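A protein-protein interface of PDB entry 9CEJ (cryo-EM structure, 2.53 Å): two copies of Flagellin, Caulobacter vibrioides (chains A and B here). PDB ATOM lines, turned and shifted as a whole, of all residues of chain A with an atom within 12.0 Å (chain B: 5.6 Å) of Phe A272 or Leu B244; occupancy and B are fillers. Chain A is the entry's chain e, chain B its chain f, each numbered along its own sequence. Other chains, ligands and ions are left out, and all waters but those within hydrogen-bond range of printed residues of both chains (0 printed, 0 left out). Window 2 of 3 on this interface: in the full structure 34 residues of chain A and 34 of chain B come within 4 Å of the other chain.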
ATOM      1  N   ASN A   4      15.979  29.668  -1.975  1.00  0.00           N
ATOM      2  CA  ASN A   4      15.674  28.584  -1.045  1.00  0.00           C
ATOM      3  C   ASN A   4      16.095  29.050   0.345  1.00  0.00           C
ATOM      4  O   ASN A   4      17.081  28.579   0.911  1.00  0.00           O
ATOM      5  CB  ASN A   4      16.389  27.295  -1.451  1.00  0.00           C
ATOM      6  CG  ASN A   4      16.062  26.865  -2.866  1.00  0.00           C
ATOM      7  OD1 ASN A   4      15.050  27.276  -3.432  1.00  0.00           O
ATOM      8  ND2 ASN A   4      16.927  26.046  -3.453  1.00  0.00           N
ATOM      9  N   SER A   5      15.341  30.001   0.889  1.00  0.00           N
ATOM     10  CA  SER A   5      15.663  30.632   2.160  1.00  0.00           C
ATOM     11  C   SER A   5      14.803  30.060   3.278  1.00  0.00           C
ATOM     12  O   SER A   5      13.618  29.779   3.085  1.00  0.00           O
ATOM     13  CB  SER A   5      15.459  32.146   2.085  1.00  0.00           C
ATOM     14  OG  SER A   5      14.116  32.485   2.385  1.00  0.00           O
ATOM     15  N   ILE A   6      15.419  29.888   4.452  1.00  0.00           N
ATOM     16  CA  ILE A   6      14.685  29.529   5.662  1.00  0.00           C
ATOM     17  C   ILE A   6      14.099  30.734   6.386  1.00  0.00           C
ATOM     18  O   ILE A   6      13.292  30.553   7.312  1.00  0.00           O
ATOM     19  CB  ILE A   6      15.594  28.740   6.624  1.00  0.00           C
ATOM     20  CG1 ILE A   6      16.780  29.601   7.056  1.00  0.00           C
ATOM     21  CG2 ILE A   6      16.077  27.454   5.981  1.00  0.00           C
ATOM     22  CD1 ILE A   6      17.597  28.996   8.170  1.00  0.00           C
ATOM     23  N   ASN A   7      14.470  31.957   5.996  1.00  0.00           N
ATOM     24  CA  ASN A   7      14.046  33.160   6.709  1.00  0.00           C
ATOM     25  C   ASN A   7      12.745  33.760   6.185  1.00  0.00           C
ATOM     26  O   ASN A   7      11.996  34.367   6.958  1.00  0.00           O
ATOM     27  CB  ASN A   7      15.149  34.221   6.650  1.00  0.00           C
ATOM     28  CG  ASN A   7      16.414  33.788   7.357  1.00  0.00           C
ATOM     29  OD1 ASN A   7      16.434  33.608   8.574  1.00  0.00           O
ATOM     30  ND2 ASN A   7      17.478  33.606   6.592  1.00  0.00           N
ATOM     31  N   SER A 264       7.007  24.364   2.317  1.00  0.00           N
ATOM     32  CA  SER A 264       8.123  24.457   1.375  1.00  0.00           C
ATOM     33  C   SER A 264       9.493  24.459   2.051  1.00  0.00           C
ATOM     34  O   SER A 264      10.471  23.996   1.450  1.00  0.00           O
ATOM     35  CB  SER A 264       7.977  25.716   0.522  1.00  0.00           C
ATOM     36  OG  SER A 264       7.605  26.826   1.319  1.00  0.00           O
ATOM     37  N   SER A 265       9.598  24.968   3.280  1.00  0.00           N
ATOM     38  CA  SER A 265      10.912  25.183   3.882  1.00  0.00           C
ATOM     39  C   SER A 265      11.636  23.887   4.238  1.00  0.00           C
ATOM     40  O   SER A 265      12.864  23.901   4.373  1.00  0.00           O
ATOM     41  CB  SER A 265      10.783  26.063   5.127  1.00  0.00           C
ATOM     42  OG  SER A 265      10.057  25.407   6.147  1.00  0.00           O
ATOM     43  N   SER A 266      10.916  22.774   4.386  1.00  0.00           N
ATOM     44  CA  SER A 266      11.513  21.558   4.933  1.00  0.00           C
ATOM     45  C   SER A 266      12.542  20.914   4.011  1.00  0.00           C
ATOM     46  O   SER A 266      13.374  20.137   4.490  1.00  0.00           O
ATOM     47  CB  SER A 266      10.415  20.546   5.263  1.00  0.00           C
ATOM     48  OG  SER A 266       9.551  21.044   6.268  1.00  0.00           O
ATOM     49  N   SER A 267      12.505  21.206   2.709  1.00  0.00           N
ATOM     50  CA  SER A 267      13.373  20.507   1.763  1.00  0.00           C
ATOM     51  C   SER A 267      14.850  20.795   2.008  1.00  0.00           C
ATOM     52  O   SER A 267      15.706  19.978   1.651  1.00  0.00           O
ATOM     53  CB  SER A 267      12.991  20.882   0.332  1.00  0.00           C
ATOM     54  OG  SER A 267      11.747  20.305  -0.027  1.00  0.00           O
ATOM     55  N   ILE A 268      15.172  21.948   2.599  1.00  0.00           N
ATOM     56  CA  ILE A 268      16.568  22.285   2.868  1.00  0.00           C
ATOM     57  C   ILE A 268      17.173  21.336   3.895  1.00  0.00           C
ATOM     58  O   ILE A 268      18.383  21.077   3.880  1.00  0.00           O
ATOM     59  CB  ILE A 268      16.664  23.756   3.315  1.00  0.00           C
ATOM     60  CG1 ILE A 268      16.197  24.672   2.186  1.00  0.00           C
ATOM     61  CG2 ILE A 268      18.082  24.119   3.725  1.00  0.00           C
ATOM     62  CD1 ILE A 268      16.010  26.098   2.608  1.00  0.00           C
ATOM     63  N   LEU A 269      16.344  20.779   4.781  1.00  0.00           N
ATOM     64  CA  LEU A 269      16.852  19.910   5.838  1.00  0.00           C
ATOM     65  C   LEU A 269      17.511  18.657   5.277  1.00  0.00           C
ATOM     66  O   LEU A 269      18.445  18.123   5.886  1.00  0.00           O
ATOM     67  CB  LEU A 269      15.712  19.529   6.781  1.00  0.00           C
ATOM     68  CG  LEU A 269      15.454  20.450   7.971  1.00  0.00           C
ATOM     69  CD1 LEU A 269      14.193  20.013   8.682  1.00  0.00           C
ATOM     70  CD2 LEU A 269      16.634  20.439   8.921  1.00  0.00           C
ATOM     71  N   SER A 270      17.040  18.172   4.125  1.00  0.00           N
ATOM     72  CA  SER A 270      17.635  16.985   3.520  1.00  0.00           C
ATOM     73  C   SER A 270      19.058  17.239   3.044  1.00  0.00           C
ATOM     74  O   SER A 270      19.865  16.305   2.983  1.00  0.00           O
ATOM     75  CB  SER A 270      16.776  16.507   2.351  1.00  0.00           C
ATOM     76  OG  SER A 270      15.497  16.096   2.794  1.00  0.00           O
ATOM     77  N   LEU A 271      19.382  18.484   2.694  1.00  0.00           N
ATOM     78  CA  LEU A 271      20.691  18.812   2.147  1.00  0.00           C
ATOM     79  C   LEU A 271      21.775  18.928   3.210  1.00  0.00           C
ATOM     80  O   LEU A 271      22.957  18.988   2.859  1.00  0.00           O
ATOM     81  CB  LEU A 271      20.611  20.115   1.353  1.00  0.00           C
ATOM     82  CG  LEU A 271      19.510  20.179   0.294  1.00  0.00           C
ATOM     83  CD1 LEU A 271      19.601  21.474  -0.481  1.00  0.00           C
ATOM     84  CD2 LEU A 271      19.601  18.991  -0.645  1.00  0.00           C
ATOM     85  N   PHE A 272      21.410  18.958   4.486  1.00  0.00           N
ATOM     86  CA  PHE A 272      22.393  19.081   5.553  1.00  0.00           C
ATOM     87  C   PHE A 272      22.401  17.835   6.431  1.00  0.00           C
ATOM     88  O   PHE A 272      23.216  16.934   6.238  1.00  0.00           O
ATOM     89  CB  PHE A 272      22.113  20.324   6.398  1.00  0.00           C
ATOM     90  CG  PHE A 272      22.594  21.602   5.775  1.00  0.00           C
ATOM     91  CD1 PHE A 272      23.939  21.922   5.776  1.00  0.00           C
ATOM     92  CD2 PHE A 272      21.702  22.483   5.190  1.00  0.00           C
ATOM     93  CE1 PHE A 272      24.385  23.095   5.203  1.00  0.00           C
ATOM     94  CE2 PHE A 272      22.142  23.658   4.618  1.00  0.00           C
ATOM     95  CZ  PHE A 272      23.485  23.965   4.626  1.00  0.00           C
ATOM     96  N   LEU B  26      35.734  28.179   5.701  1.00  0.00           N
ATOM     97  CA  LEU B  26      34.801  27.282   6.377  1.00  0.00           C
ATOM     98  C   LEU B  26      34.022  27.999   7.475  1.00  0.00           C
ATOM     99  O   LEU B  26      32.814  27.777   7.632  1.00  0.00           O
ATOM    100  CB  LEU B  26      35.549  26.081   6.948  1.00  0.00           C
ATOM    101  CG  LEU B  26      34.685  24.888   7.359  1.00  0.00           C
ATOM    102  CD1 LEU B  26      33.581  24.634   6.352  1.00  0.00           C
ATOM    103  CD2 LEU B  26      35.547  23.658   7.506  1.00  0.00           C
ATOM    104  N   VAL B  29      31.316  30.017   5.735  1.00  0.00           N
ATOM    105  CA  VAL B  29      30.144  29.273   5.286  1.00  0.00           C
ATOM    106  C   VAL B  29      29.314  28.786   6.472  1.00  0.00           C
ATOM    107  O   VAL B  29      28.079  28.755   6.397  1.00  0.00           O
ATOM    108  CB  VAL B  29      30.533  28.119   4.341  1.00  0.00           C
ATOM    109  CG1 VAL B  29      31.392  27.098   5.033  1.00  0.00           C
ATOM    110  CG2 VAL B  29      29.286  27.461   3.765  1.00  0.00           C
ATOM    111  N   ILE B  33      25.490  29.444   7.527  1.00  0.00           N
ATOM    112  CA  ILE B  33      24.586  28.322   7.766  1.00  0.00           C
ATOM    113  C   ILE B  33      23.793  28.531   9.053  1.00  0.00           C
ATOM    114  O   ILE B  33      22.563  28.410   9.065  1.00  0.00           O
ATOM    115  CB  ILE B  33      25.370  26.997   7.791  1.00  0.00           C
ATOM    116  CG1 ILE B  33      25.655  26.531   6.365  1.00  0.00           C
ATOM    117  CG2 ILE B  33      24.592  25.932   8.544  1.00  0.00           C
ATOM    118  CD1 ILE B  33      26.910  25.715   6.237  1.00  0.00           C
ATOM    119  N   LEU B 237      20.853  28.399   1.125  1.00  0.00           N
ATOM    120  CA  LEU B 237      21.488  27.291   1.835  1.00  0.00           C
ATOM    121  C   LEU B 237      21.796  26.116   0.913  1.00  0.00           C
ATOM    122  O   LEU B 237      22.780  25.392   1.138  1.00  0.00           O
ATOM    123  CB  LEU B 237      20.592  26.828   2.987  1.00  0.00           C
ATOM    124  CG  LEU B 237      20.635  27.577   4.325  1.00  0.00           C
ATOM    125  CD1 LEU B 237      22.009  27.448   4.963  1.00  0.00           C
ATOM    126  CD2 LEU B 237      20.230  29.037   4.198  1.00  0.00           C
ATOM    127  N   ALA B 238      20.977  25.912  -0.123  1.00  0.00           N
ATOM    128  CA  ALA B 238      21.200  24.797  -1.035  1.00  0.00           C
ATOM    129  C   ALA B 238      22.527  24.930  -1.762  1.00  0.00           C
ATOM    130  O   ALA B 238      23.161  23.921  -2.091  1.00  0.00           O
ATOM    131  CB  ALA B 238      20.052  24.704  -2.040  1.00  0.00           C
ATOM    132  N   GLU B 240      25.001  26.629  -0.246  1.00  0.00           N
ATOM    133  CA  GLU B 240      25.972  26.600   0.844  1.00  0.00           C
ATOM    134  C   GLU B 240      26.393  25.180   1.199  1.00  0.00           C
ATOM    135  O   GLU B 240      27.514  24.969   1.677  1.00  0.00           O
ATOM    136  CB  GLU B 240      25.397  27.300   2.076  1.00  0.00           C
ATOM    137  CG  GLU B 240      24.991  28.764   1.881  1.00  0.00           C
ATOM    138  CD  GLU B 240      25.961  29.574   1.028  1.00  0.00           C
ATOM    139  OE1 GLU B 240      25.489  30.425   0.245  1.00  0.00           O
ATOM    140  OE2 GLU B 240      27.189  29.397   1.167  1.00  0.00           O
ATOM    141  N   SER B 241      25.509  24.198   0.988  1.00  0.00           N
ATOM    142  CA  SER B 241      25.822  22.830   1.402  1.00  0.00           C
ATOM    143  C   SER B 241      27.034  22.282   0.656  1.00  0.00           C
ATOM    144  O   SER B 241      27.888  21.594   1.242  1.00  0.00           O
ATOM    145  CB  SER B 241      24.612  21.929   1.166  1.00  0.00           C
ATOM    146  OG  SER B 241      23.509  22.331   1.955  1.00  0.00           O
ATOM    147  N   ALA B 242      27.142  22.604  -0.635  1.00  0.00           N
ATOM    148  CA  ALA B 242      28.237  22.075  -1.437  1.00  0.00           C
ATOM    149  C   ALA B 242      29.571  22.658  -0.999  1.00  0.00           C
ATOM    150  O   ALA B 242      30.556  21.924  -0.854  1.00  0.00           O
ATOM    151  CB  ALA B 242      27.988  22.365  -2.916  1.00  0.00           C
ATOM    152  N   LYS B 243      29.617  23.972  -0.767  1.00  0.00           N
ATOM    153  CA  LYS B 243      30.842  24.573  -0.259  1.00  0.00           C
ATOM    154  C   LYS B 243      31.175  24.062   1.132  1.00  0.00           C
ATOM    155  O   LYS B 243      32.351  23.893   1.453  1.00  0.00           O
ATOM    156  CB  LYS B 243      30.738  26.098  -0.258  1.00  0.00           C
ATOM    157  CG  LYS B 243      30.668  26.717  -1.642  1.00  0.00           C
ATOM    158  CD  LYS B 243      30.733  28.235  -1.571  1.00  0.00           C
ATOM    159  CE  LYS B 243      29.431  28.822  -1.057  1.00  0.00           C
ATOM    160  NZ  LYS B 243      29.429  30.311  -1.081  1.00  0.00           N
ATOM    161  N   LEU B 244      30.166  23.757   1.951  1.00  0.00           N
ATOM    162  CA  LEU B 244      30.448  23.196   3.268  1.00  0.00           C
ATOM    163  C   LEU B 244      31.187  21.868   3.144  1.00  0.00           C
ATOM    164  O   LEU B 244      32.267  21.681   3.728  1.00  0.00           O
ATOM    165  CB  LEU B 244      29.142  23.013   4.044  1.00  0.00           C
ATOM    166  CG  LEU B 244      29.173  22.214   5.353  1.00  0.00           C
ATOM    167  CD1 LEU B 244      30.330  22.633   6.250  1.00  0.00           C
ATOM    168  CD2 LEU B 244      27.847  22.308   6.088  1.00  0.00           C
ATOM    169  N   GLN B 245      30.629  20.936   2.367  1.00  0.00           N
ATOM    170  CA  GLN B 245      31.264  19.624   2.262  1.00  0.00           C
ATOM    171  C   GLN B 245      32.621  19.713   1.569  1.00  0.00           C
ATOM    172  O   GLN B 245      33.586  19.042   1.974  1.00  0.00           O
ATOM    173  CB  GLN B 245      30.342  18.650   1.533  1.00  0.00           C
ATOM    174  CG  GLN B 245      28.914  18.652   2.047  1.00  0.00           C
ATOM    175  CD  GLN B 245      28.130  17.451   1.567  1.00  0.00           C
ATOM    176  OE1 GLN B 245      26.934  17.541   1.293  1.00  0.00           O
ATOM    177  NE2 GLN B 245      28.802  16.312   1.471  1.00  0.00           N
ATOM    178  N   SER B 246      32.728  20.566   0.547  1.00  0.00           N
ATOM    179  CA  SER B 246      33.988  20.693  -0.176  1.00  0.00           C
ATOM    180  C   SER B 246      35.069  21.299   0.705  1.00  0.00           C
ATOM    181  O   SER B 246      36.227  20.878   0.656  1.00  0.00           O
ATOM    182  CB  SER B 246      33.784  21.536  -1.433  1.00  0.00           C
ATOM    183  OG  SER B 246      35.013  22.075  -1.882  1.00  0.00           O
ATOM    184  N   LEU B 247      34.712  22.297   1.519  1.00  0.00           N
ATOM    185  CA  LEU B 247      35.688  22.890   2.422  1.00  0.00           C
ATOM    186  C   LEU B 247      36.088  21.932   3.534  1.00  0.00           C
ATOM    187  O   LEU B 247      37.233  21.972   3.988  1.00  0.00           O
ATOM    188  CB  LEU B 247      35.148  24.195   3.006  1.00  0.00           C
ATOM    189  CG  LEU B 247      35.009  25.351   2.014  1.00  0.00           C
ATOM    190  CD1 LEU B 247      34.083  26.419   2.565  1.00  0.00           C
ATOM    191  CD2 LEU B 247      36.368  25.935   1.671  1.00  0.00           C
ATOM    192  N   GLN B 248      35.183  21.053   3.972  1.00  0.00           N
ATOM    193  CA  GLN B 248      35.599  20.046   4.947  1.00  0.00           C
ATOM    194  C   GLN B 248      36.624  19.091   4.343  1.00  0.00           C
ATOM    195  O   GLN B 248      37.660  18.789   4.964  1.00  0.00           O
ATOM    196  CB  GLN B 248      34.384  19.277   5.464  1.00  0.00           C
ATOM    197  CG  GLN B 248      33.699  19.929   6.653  1.00  0.00           C
ATOM    198  CD  GLN B 248      32.264  19.473   6.825  1.00  0.00           C
ATOM    199  OE1 GLN B 248      31.796  18.581   6.119  1.00  0.00           O
ATOM    200  NE2 GLN B 248      31.557  20.086   7.767  1.00  0.00           N
ATOM    201  N   THR B 249      36.371  18.633   3.114  1.00  0.00           N
ATOM    202  CA  THR B 249      37.346  17.772   2.448  1.00  0.00           C
ATOM    203  C   THR B 249      38.664  18.506   2.212  1.00  0.00           C
ATOM    204  O   THR B 249      39.749  17.932   2.383  1.00  0.00           O
ATOM    205  CB  THR B 249      36.773  17.263   1.126  1.00  0.00           C
ATOM    206  OG1 THR B 249      35.464  16.725   1.349  1.00  0.00           O
ATOM    207  CG2 THR B 249      37.665  16.189   0.536  1.00  0.00           C
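Asn A4 touches Leu B237.
ND2 of Asn A4 touches CB of Ala B238, at 3.7 Å.
Ile A268 touches Leu B237.
CD1 of Leu A271 touches CB of Ala B238, 3.6 Å away.
Leu A271 touches Ser B241.
Ile B33 touches Phe A272.
CZ of Phe A272 touches CD1 of Leu B237 (3.8 Å).
CZ of Phe A272 touches OG of Ser B241 (3.1 Å).
CE1 of Phe A272 touches CD2 of Leu B244, 3.7 Å away.
Of the 15 printed residues of chain B, 5 touch a printed residue of chain A.
Printed residues of chain A that touch a printed residue of chain B: Asn A4, Ile A268, Leu A271 and Phe A272.
Hydrophobic or aromatic side chains of chain A that line the printed part of chain B: Ile A268, Leu A271 and Phe A272.
Among the printed residues, 9 pairs touch across the chains.
No position is printed for both chains.
Phe A272 touches just these residues of chain B: Ile B33 (3.8 Å), Leu B237 (3.8 Å), Ser B241 (3.1 Å) and Leu B244 (3.7 Å).
Leu B244 touches just one residue of chain A: Phe A272 (3.7 Å).
Leu B237 touches just these residues of chain A: Asn A4 (3.8 Å), Ile A268 (3.8 Å) and Phe A272 (3.8 Å).
Of chain A, only Asn A4 and Leu A271 come within 4 Å of Ala B238.
Ala B242 touches none of the printed residues of chain A.
No residue of chain A comes within 4 Å of Ser B246.
No residue of chain A comes within 4 Å of Leu B247.
No residue of chain A comes within 4 Å of Gln B248.
Of the printed residues of chain B, Asn A4 touches Leu B237 (3.8 Å) and Ala B238 (3.7 Å).
Of the printed residues of chain B, Ile A268 touches Leu B237.
Printed residues of chain B within 4 Å of Leu A271: Ala B238 (3.6 Å) and Ser B241 (3.5 Å).
Glu B240 touches none of the printed residues of chain A.
The nearest residue of chain A that does not touch Leu B244 is Leu A271 (6.7 Å).
The backbone carbonyl oxygen (O) of Leu B237 lies within hydrogen-bond range of the side-chain hydroxyl (OG) of Ser B241, 3.3 Å away.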
